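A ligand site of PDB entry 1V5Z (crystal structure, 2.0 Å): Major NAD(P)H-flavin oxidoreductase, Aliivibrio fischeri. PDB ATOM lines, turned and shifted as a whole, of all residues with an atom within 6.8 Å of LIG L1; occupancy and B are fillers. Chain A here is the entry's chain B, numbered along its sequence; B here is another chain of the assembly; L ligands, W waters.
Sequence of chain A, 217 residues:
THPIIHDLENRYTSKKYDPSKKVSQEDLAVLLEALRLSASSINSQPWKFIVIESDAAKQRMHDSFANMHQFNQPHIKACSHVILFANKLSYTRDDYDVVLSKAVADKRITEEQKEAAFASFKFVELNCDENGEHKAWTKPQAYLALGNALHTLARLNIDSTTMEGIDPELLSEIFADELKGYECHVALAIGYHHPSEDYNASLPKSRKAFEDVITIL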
ATOM      1  N   SER A  40      10.482  11.744  11.198  1.00  0.00           N
ATOM      2  CA  SER A  40      10.754  12.245   9.851  1.00  0.00           C
ATOM      3  C   SER A  40      12.241  12.247   9.660  1.00  0.00           C
ATOM      4  O   SER A  40      12.979  12.210  10.630  1.00  0.00           O
ATOM      5  CB  SER A  40      10.193  13.675   9.662  1.00  0.00           C
ATOM      6  OG  SER A  40      10.735  14.578  10.616  1.00  0.00           O
ATOM      7  N   SER A  41      12.693  12.272   8.399  1.00  0.00           N
ATOM      8  CA  SER A  41      14.120  12.272   8.068  1.00  0.00           C
ATOM      9  C   SER A  41      14.778  13.448   8.744  1.00  0.00           C
ATOM     10  O   SER A  41      14.281  14.555   8.658  1.00  0.00           O
ATOM     11  CB  SER A  41      14.347  12.380   6.566  1.00  0.00           C
ATOM     12  OG  SER A  41      13.463  11.520   5.882  1.00  0.00           O
ATOM     13  N   ILE A  42      15.922  13.197   9.350  1.00  0.00           N
ATOM     14  CA  ILE A  42      16.699  14.172  10.118  1.00  0.00           C
ATOM     15  C   ILE A  42      15.914  15.037  11.109  1.00  0.00           C
ATOM     16  O   ILE A  42      16.440  16.028  11.615  1.00  0.00           O
ATOM     17  CB  ILE A  42      17.673  15.006   9.228  1.00  0.00           C
ATOM     18  CG1 ILE A  42      16.933  15.983   8.298  1.00  0.00           C
ATOM     19  CG2 ILE A  42      18.573  14.074   8.426  1.00  0.00           C
ATOM     20  CD1 ILE A  42      17.876  16.951   7.614  1.00  0.00           C
ATOM     21  N   ASN A  43      14.716  14.566  11.490  1.00  0.00           N
ATOM     22  CA  ASN A  43      13.816  15.269  12.416  1.00  0.00           C
ATOM     23  C   ASN A  43      13.460  16.626  11.799  1.00  0.00           C
ATOM     24  O   ASN A  43      13.216  17.603  12.491  1.00  0.00           O
ATOM     25  CB  ASN A  43      14.452  15.451  13.810  1.00  0.00           C
ATOM     26  CG  ASN A  43      13.406  15.675  14.919  1.00  0.00           C
ATOM     27  OD1 ASN A  43      12.256  15.280  14.783  1.00  0.00           O
ATOM     28  ND2 ASN A  43      13.815  16.315  16.009  1.00  0.00           N
ATOM     29  N   SER A 120      23.993  16.910   9.169  1.00  0.00           N
ATOM     30  CA  SER A 120      22.889  16.021   8.826  1.00  0.00           C
ATOM     31  C   SER A 120      22.114  16.619   7.662  1.00  0.00           C
ATOM     32  O   SER A 120      21.463  15.907   6.900  1.00  0.00           O
ATOM     33  CB  SER A 120      21.959  15.839  10.022  1.00  0.00           C
ATOM     34  OG  SER A 120      22.635  15.401  11.187  1.00  0.00           O
ATOM     35  N   PHE A 123      21.782  15.533   3.758  1.00  0.00           N
ATOM     36  CA  PHE A 123      20.770  14.541   3.387  1.00  0.00           C
ATOM     37  C   PHE A 123      19.527  15.207   2.778  1.00  0.00           C
ATOM     38  O   PHE A 123      18.706  14.544   2.141  1.00  0.00           O
ATOM     39  CB  PHE A 123      20.413  13.726   4.623  1.00  0.00           C
ATOM     40  CG  PHE A 123      21.605  13.120   5.331  1.00  0.00           C
ATOM     41  CD1 PHE A 123      21.526  12.725   6.656  1.00  0.00           C
ATOM     42  CD2 PHE A 123      22.805  12.921   4.645  1.00  0.00           C
ATOM     43  CE1 PHE A 123      22.621  12.123   7.307  1.00  0.00           C
ATOM     44  CE2 PHE A 123      23.908  12.326   5.277  1.00  0.00           C
ATOM     45  CZ  PHE A 123      23.816  11.921   6.609  1.00  0.00           C
ATOM     46  N   VAL A 124      19.394  16.510   3.011  1.00  0.00           N
ATOM     47  CA  VAL A 124      18.302  17.319   2.465  1.00  0.00           C
ATOM     48  C   VAL A 124      18.770  17.872   1.131  1.00  0.00           C
ATOM     49  O   VAL A 124      18.061  17.781   0.132  1.00  0.00           O
ATOM     50  CB  VAL A 124      17.954  18.524   3.378  1.00  0.00           C
ATOM     51  CG1 VAL A 124      16.937  19.441   2.701  1.00  0.00           C
ATOM     52  CG2 VAL A 124      17.402  18.043   4.682  1.00  0.00           C
ATOM     53  N   LEU A 126      20.756  16.718  -0.874  1.00  0.00           N
ATOM     54  CA  LEU A 126      20.757  15.613  -1.831  1.00  0.00           C
ATOM     55  C   LEU A 126      19.416  15.421  -2.552  1.00  0.00           C
ATOM     56  O   LEU A 126      19.381  14.997  -3.714  1.00  0.00           O
ATOM     57  CB  LEU A 126      21.135  14.311  -1.103  1.00  0.00           C
ATOM     58  CG  LEU A 126      22.616  13.954  -0.914  1.00  0.00           C
ATOM     59  CD1 LEU A 126      23.496  15.193  -0.797  1.00  0.00           C
ATOM     60  CD2 LEU A 126      22.772  13.020   0.289  1.00  0.00           C
ATOM     61  N   ASN A 127      18.335  15.712  -1.841  1.00  0.00           N
ATOM     62  CA  ASN A 127      16.973  15.579  -2.383  1.00  0.00           C
ATOM     63  C   ASN A 127      16.422  16.969  -2.761  1.00  0.00           C
ATOM     64  O   ASN A 127      16.328  17.845  -1.902  1.00  0.00           O
ATOM     65  CB  ASN A 127      16.078  14.904  -1.343  1.00  0.00           C
ATOM     66  CG  ASN A 127      16.609  13.547  -0.903  1.00  0.00           C
ATOM     67  OD1 ASN A 127      16.458  12.549  -1.615  1.00  0.00           O
ATOM     68  ND2 ASN A 127      17.215  13.498   0.278  1.00  0.00           N
ATOM     69  N   TRP A 137      10.592  15.124  -1.617  1.00  0.00           N
ATOM     70  CA  TRP A 137      11.127  14.526  -0.407  1.00  0.00           C
ATOM     71  C   TRP A 137      10.260  14.848   0.842  1.00  0.00           C
ATOM     72  O   TRP A 137      10.175  14.042   1.776  1.00  0.00           O
ATOM     73  CB  TRP A 137      12.567  15.032  -0.238  1.00  0.00           C
ATOM     74  CG  TRP A 137      13.227  14.727   1.073  1.00  0.00           C
ATOM     75  CD1 TRP A 137      13.743  13.506   1.480  1.00  0.00           C
ATOM     76  CD2 TRP A 137      13.462  15.644   2.152  1.00  0.00           C
ATOM     77  NE1 TRP A 137      14.281  13.625   2.741  1.00  0.00           N
ATOM     78  CE2 TRP A 137      14.113  14.920   3.183  1.00  0.00           C
ATOM     79  CE3 TRP A 137      13.181  17.005   2.350  1.00  0.00           C
ATOM     80  CZ2 TRP A 137      14.489  15.512   4.390  1.00  0.00           C
ATOM     81  CZ3 TRP A 137      13.548  17.596   3.553  1.00  0.00           C
ATOM     82  CH2 TRP A 137      14.200  16.848   4.567  1.00  0.00           C
ATOM     83  N   GLN A 141       7.132  12.459   3.830  1.00  0.00           N
ATOM     84  CA  GLN A 141       7.216  12.631   5.287  1.00  0.00           C
ATOM     85  C   GLN A 141       5.829  12.898   5.851  1.00  0.00           C
ATOM     86  O   GLN A 141       5.476  12.407   6.924  1.00  0.00           O
ATOM     87  CB  GLN A 141       8.122  13.802   5.696  1.00  0.00           C
ATOM     88  CG  GLN A 141       9.497  13.880   5.026  1.00  0.00           C
ATOM     89  CD  GLN A 141      10.345  12.654   5.251  1.00  0.00           C
ATOM     90  OE1 GLN A 141      10.592  12.262   6.378  1.00  0.00           O
ATOM     91  NE2 GLN A 141      10.799  12.041   4.160  1.00  0.00           N
ATOM     92  N   THR B  13      14.565   6.309  17.553  1.00  0.00           N
ATOM     93  CA  THR B  13      15.413   5.698  16.541  1.00  0.00           C
ATOM     94  C   THR B  13      16.622   5.066  17.218  1.00  0.00           C
ATOM     95  O   THR B  13      17.484   5.745  17.781  1.00  0.00           O
ATOM     96  CB  THR B  13      15.819   6.731  15.454  1.00  0.00           C
ATOM     97  OG1 THR B  13      14.637   7.150  14.731  1.00  0.00           O
ATOM     98  CG2 THR B  13      16.829   6.119  14.449  1.00  0.00           C
ATOM     99  N   LYS B  15      20.166   3.489  17.661  1.00  0.00           N
ATOM    100  CA  LYS B  15      21.462   3.725  17.024  1.00  0.00           C
ATOM    101  C   LYS B  15      22.473   2.588  17.250  1.00  0.00           C
ATOM    102  O   LYS B  15      23.629   2.725  16.893  1.00  0.00           O
ATOM    103  CB  LYS B  15      22.068   5.036  17.526  1.00  0.00           C
ATOM    104  CG  LYS B  15      21.218   6.276  17.275  1.00  0.00           C
ATOM    105  CD  LYS B  15      21.081   6.597  15.788  1.00  0.00           C
ATOM    106  CE  LYS B  15      20.233   7.842  15.559  1.00  0.00           C
ATOM    107  NZ  LYS B  15      20.067   8.160  14.114  1.00  0.00           N
ATOM    108  N   HIS B  69      26.437   5.698   2.554  1.00  0.00           N
ATOM    109  CA  HIS B  69      25.722   5.609   3.808  1.00  0.00           C
ATOM    110  C   HIS B  69      26.156   4.479   4.707  1.00  0.00           C
ATOM    111  O   HIS B  69      25.334   3.808   5.322  1.00  0.00           O
ATOM    112  CB  HIS B  69      24.215   5.537   3.535  1.00  0.00           C
ATOM    113  CG  HIS B  69      23.724   6.651   2.669  1.00  0.00           C
ATOM    114  ND1 HIS B  69      24.104   7.966   2.854  1.00  0.00           N
ATOM    115  CD2 HIS B  69      22.892   6.652   1.596  1.00  0.00           C
ATOM    116  CE1 HIS B  69      23.519   8.717   1.938  1.00  0.00           C
ATOM    117  NE2 HIS B  69      22.781   7.948   1.169  1.00  0.00           N
ATOM    118  N   PHE B  71      27.157   4.568   7.549  1.00  0.00           N
ATOM    119  CA  PHE B  71      26.819   4.811   8.944  1.00  0.00           C
ATOM    120  C   PHE B  71      25.626   3.924   9.342  1.00  0.00           C
ATOM    121  O   PHE B  71      25.434   3.626  10.518  1.00  0.00           O
ATOM    122  CB  PHE B  71      26.524   6.295   9.190  1.00  0.00           C
ATOM    123  CG  PHE B  71      25.240   6.808   8.547  1.00  0.00           C
ATOM    124  CD1 PHE B  71      24.093   7.006   9.313  1.00  0.00           C
ATOM    125  CD2 PHE B  71      25.191   7.090   7.197  1.00  0.00           C
ATOM    126  CE1 PHE B  71      22.920   7.485   8.727  1.00  0.00           C
ATOM    127  CE2 PHE B  71      24.009   7.579   6.605  1.00  0.00           C
ATOM    128  CZ  PHE B  71      22.880   7.769   7.381  1.00  0.00           C
ATOM    129  N   ASN B  72      24.866   3.483   8.342  1.00  0.00           N
ATOM    130  CA  ASN B  72      23.717   2.620   8.554  1.00  0.00           C
ATOM    131  C   ASN B  72      24.076   1.137   8.438  1.00  0.00           C
ATOM    132  O   ASN B  72      23.314   0.262   8.852  1.00  0.00           O
ATOM    133  CB  ASN B  72      22.647   2.933   7.502  1.00  0.00           C
ATOM    134  CG  ASN B  72      21.781   4.125   7.889  1.00  0.00           C
ATOM    135  OD1 ASN B  72      21.605   4.422   9.069  1.00  0.00           O
ATOM    136  ND2 ASN B  72      21.231   4.799   6.892  1.00  0.00           N
ATOM    137  N   THR B 162      14.622   3.563  11.079  1.00  0.00           N
ATOM    138  CA  THR B 162      14.152   3.868   9.732  1.00  0.00           C
ATOM    139  C   THR B 162      15.387   4.301   8.973  1.00  0.00           C
ATOM    140  O   THR B 162      16.256   4.986   9.516  1.00  0.00           O
ATOM    141  CB  THR B 162      13.094   5.008   9.718  1.00  0.00           C
ATOM    142  OG1 THR B 162      11.991   4.654  10.578  1.00  0.00           O
ATOM    143  CG2 THR B 162      12.557   5.185   8.310  1.00  0.00           C
ATOM    144  N   MET B 163      15.491   3.882   7.717  1.00  0.00           N
ATOM    145  CA  MET B 163      16.674   4.215   6.931  1.00  0.00           C
ATOM    146  C   MET B 163      16.419   4.689   5.516  1.00  0.00           C
ATOM    147  O   MET B 163      15.891   3.945   4.683  1.00  0.00           O
ATOM    148  CB  MET B 163      17.643   3.024   6.914  1.00  0.00           C
ATOM    149  CG  MET B 163      18.267   2.676   8.273  1.00  0.00           C
ATOM    150  SD  MET B 163      19.320   1.183   8.308  1.00  0.00           S
ATOM    151  CE  MET B 163      18.204   0.068   7.580  1.00  0.00           C
ATOM    152  N   GLU B 164      16.729   5.949   5.268  1.00  0.00           N
ATOM    153  CA  GLU B 164      16.614   6.527   3.929  1.00  0.00           C
ATOM    154  C   GLU B 164      18.047   6.590   3.411  1.00  0.00           C
ATOM    155  O   GLU B 164      18.280   6.848   2.228  1.00  0.00           O
ATOM    156  CB  GLU B 164      15.988   7.932   3.973  1.00  0.00           C
ATOM    157  CG  GLU B 164      14.627   8.019   3.311  1.00  0.00           C
ATOM    158  CD  GLU B 164      14.049   9.454   3.336  1.00  0.00           C
ATOM    159  OE1 GLU B 164      14.779  10.404   3.663  1.00  0.00           O
ATOM    160  OE2 GLU B 164      12.855   9.623   3.025  1.00  0.00           O
ATOM    161  N   GLY B 165      19.007   6.372   4.306  1.00  0.00           N
ATOM    162  CA  GLY B 165      20.404   6.373   3.940  1.00  0.00           C
ATOM    163  C   GLY B 165      20.773   4.987   3.418  1.00  0.00           C
ATOM    164  O   GLY B 165      21.521   4.263   4.047  1.00  0.00           O
ATOM    165  N   ILE B 166      20.172   4.635   2.274  1.00  0.00           N
ATOM    166  CA  ILE B 166      20.389   3.370   1.581  1.00  0.00           C
ATOM    167  C   ILE B 166      20.719   3.682   0.108  1.00  0.00           C
ATOM    168  O   ILE B 166      20.589   4.831  -0.332  1.00  0.00           O
ATOM    169  CB  ILE B 166      19.123   2.450   1.650  1.00  0.00           C
ATOM    170  CG1 ILE B 166      17.951   3.116   0.928  1.00  0.00           C
ATOM    171  CG2 ILE B 166      18.757   2.157   3.126  1.00  0.00           C
ATOM    172  CD1 ILE B 166      16.706   2.277   0.846  1.00  0.00           C
HETATM  173  C1  LIG L   1      19.524  10.457   8.650  1.00  0.00           C
HETATM  174  C2  LIG L   1      18.909  10.715  10.071  1.00  0.00           C
HETATM  175  O1  LIG L   1      19.696  10.639  10.993  1.00  0.00           O
HETATM  176  O2  LIG L   1      17.699  10.956  10.052  1.00  0.00           O
HETATM  177  C3  LIG L   1      18.568  10.568   7.498  1.00  0.00           C
HETATM  178  C4  LIG L   1      19.052  10.324   6.070  1.00  0.00           C
HETATM  179  C5  LIG L   1      20.400   9.971   5.828  1.00  0.00           C
HETATM  180  C6  LIG L   1      20.857   9.745   4.585  1.00  0.00           C
HETATM  181  C7  LIG L   1      20.034   9.843   3.486  1.00  0.00           C
HETATM  182  C8  LIG L   1      18.614  10.204   3.637  1.00  0.00           C
HETATM  183  C9  LIG L   1      18.129  10.443   5.043  1.00  0.00           C
HETATM  184  O3  LIG L   1      16.751  10.813   5.324  1.00  0.00           O
HETATM  185  N1  LG2 L   2      18.007   7.510  11.154  1.00  0.00           N
HETATM  186  C1  LG2 L   2      19.166   6.819  10.948  1.00  0.00           C
HETATM  187  O1  LG2 L   2      20.039   6.732  11.800  1.00  0.00           O
HETATM  188  N2  LG2 L   2      19.442   6.669   9.618  1.00  0.00           N
HETATM  189  C2  LG2 L   2      18.608   6.963   8.532  1.00  0.00           C
HETATM  190  O2  LG2 L   2      19.045   6.708   7.396  1.00  0.00           O
HETATM  191  C3  LG2 L   2      17.400   7.613   8.891  1.00  0.00           C
HETATM  192  N3  LG2 L   2      16.490   7.877   7.865  1.00  0.00           N
HETATM  193  C4  LG2 L   2      15.219   8.262   8.147  1.00  0.00           C
HETATM  194  C5  LG2 L   2      14.255   8.196   7.171  1.00  0.00           C
HETATM  195  C6  LG2 L   2      12.951   8.522   7.472  1.00  0.00           C
HETATM  196  C7  LG2 L   2      11.843   8.614   6.400  1.00  0.00           C
HETATM  197  C8  LG2 L   2      12.604   8.798   8.778  1.00  0.00           C
HETATM  198  C9  LG2 L   2      11.171   8.893   9.220  1.00  0.00           C
HETATM  199  C10 LG2 L   2      13.560   8.789   9.742  1.00  0.00           C
HETATM  200  C11 LG2 L   2      14.863   8.516   9.453  1.00  0.00           C
HETATM  201  N4  LG2 L   2      15.789   8.338  10.492  1.00  0.00           N
HETATM  202  C12 LG2 L   2      17.025   7.823  10.231  1.00  0.00           C
HETATM  203  C13 LG2 L   2      15.501   8.580  11.821  1.00  0.00           C
HETATM  204  C14 LG2 L   2      15.152  10.057  12.144  1.00  0.00           C
HETATM  205  O3  LG2 L   2      16.320  10.789  12.413  1.00  0.00           O
HETATM  206  C15 LG2 L   2      14.198  10.082  13.356  1.00  0.00           C
HETATM  207  O4  LG2 L   2      12.992   9.384  13.063  1.00  0.00           O
HETATM  208  C16 LG2 L   2      13.931  11.561  13.817  1.00  0.00           C
HETATM  209  O5  LG2 L   2      15.209  12.164  14.228  1.00  0.00           O
HETATM  210  C17 LG2 L   2      12.997  11.645  15.015  1.00  0.00           C
HETATM  211  O6  LG2 L   2      13.508  10.902  16.175  1.00  0.00           O
HETATM  212  P1  LG2 L   2      12.847   9.493  16.750  1.00  0.00           P
HETATM  213  O7  LG2 L   2      13.984   9.209  17.638  1.00  0.00           O
HETATM  214  O8  LG2 L   2      12.694   8.715  15.491  1.00  0.00           O
HETATM  215  O9  LG2 L   2      11.609  10.075  17.276  1.00  0.00           O
HETATM  216  O   HOH W   1      19.318  13.064  12.738  1.00  0.00           O
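OE1 of Glu 164 of chain B sits at hydrogen-bond distance from O3 of LIG L1 (2.6 Å).
The backbone NH of Ile 42 is in hydrogen-bond range of an oxygen (O2) of LIG L1.
The side-chain hydroxyl (OG) of Ser 41 sits close to an oxygen (O3) of LIG L1 (3.4 Å).
The backbone NH of Glu 164 of chain B lies within hydrogen-bond range of an oxygen (O2) of LG2 L2 (3.2 Å).
An oxygen (O2) of LG2 L2 is in hydrogen-bond range of the backbone NH of Gly 165 of chain B, 3.1 Å away.
NZ of Lys 15 of chain B lies within hydrogen-bond range of O1 of LG2 L2 (2.7 Å).
The side-chain amide nitrogen (ND2) of Asn 72 of chain B sits at hydrogen-bond distance from an oxygen (O2) of LG2 L2, at 2.9 Å.
N of Thr 13 of chain B sits at hydrogen-bond distance from O7 of LG2 L2.
An oxygen (O8) of LG2 L2 sits at hydrogen-bond distance from the side-chain hydroxyl (OG1) of Thr 13 of chain B (2.6 Å).
O2 of LIG L1 lies within hydrogen-bond range of O3 of LG2 L2, at 2.7 Å.
OE1 of Glu 164 of chain B sits at hydrogen-bond distance from OG of Ser 41 (2.8 Å).
OE1 of Glu 164 of chain B lies within hydrogen-bond range of NE1 of Trp 137 (3.4 Å).
The side-chain amide nitrogen (NE2) of Gln 141 lies within hydrogen-bond range of the side-chain carboxylate (OE2) of Glu 164 of chain B, at 3.4 Å.
O of Phe 123 sits at hydrogen-bond distance from ND2 of Asn 127.
The backbone NH (N) of Ser 41 is in hydrogen-bond range of the side-chain amide oxygen (OE1) of Gln 141, at 2.9 Å.
The backbone carbonyl oxygen of Gly 165 of chain B is in hydrogen-bond range of the side-chain amide nitrogen of Asn 72 of chain B (2.9 Å).
CD1 of Phe 123 touches C5 of LIG L1 (3.1 Å).
His 69 of chain B touches LIG L1.
Phe 71 of chain B touches LIG L1.
CA of Gly 165 of chain B touches C6 of LIG L1, at 3.5 Å.
Of the 21 residues printed, 7 come within 4 Å of LIG L1.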
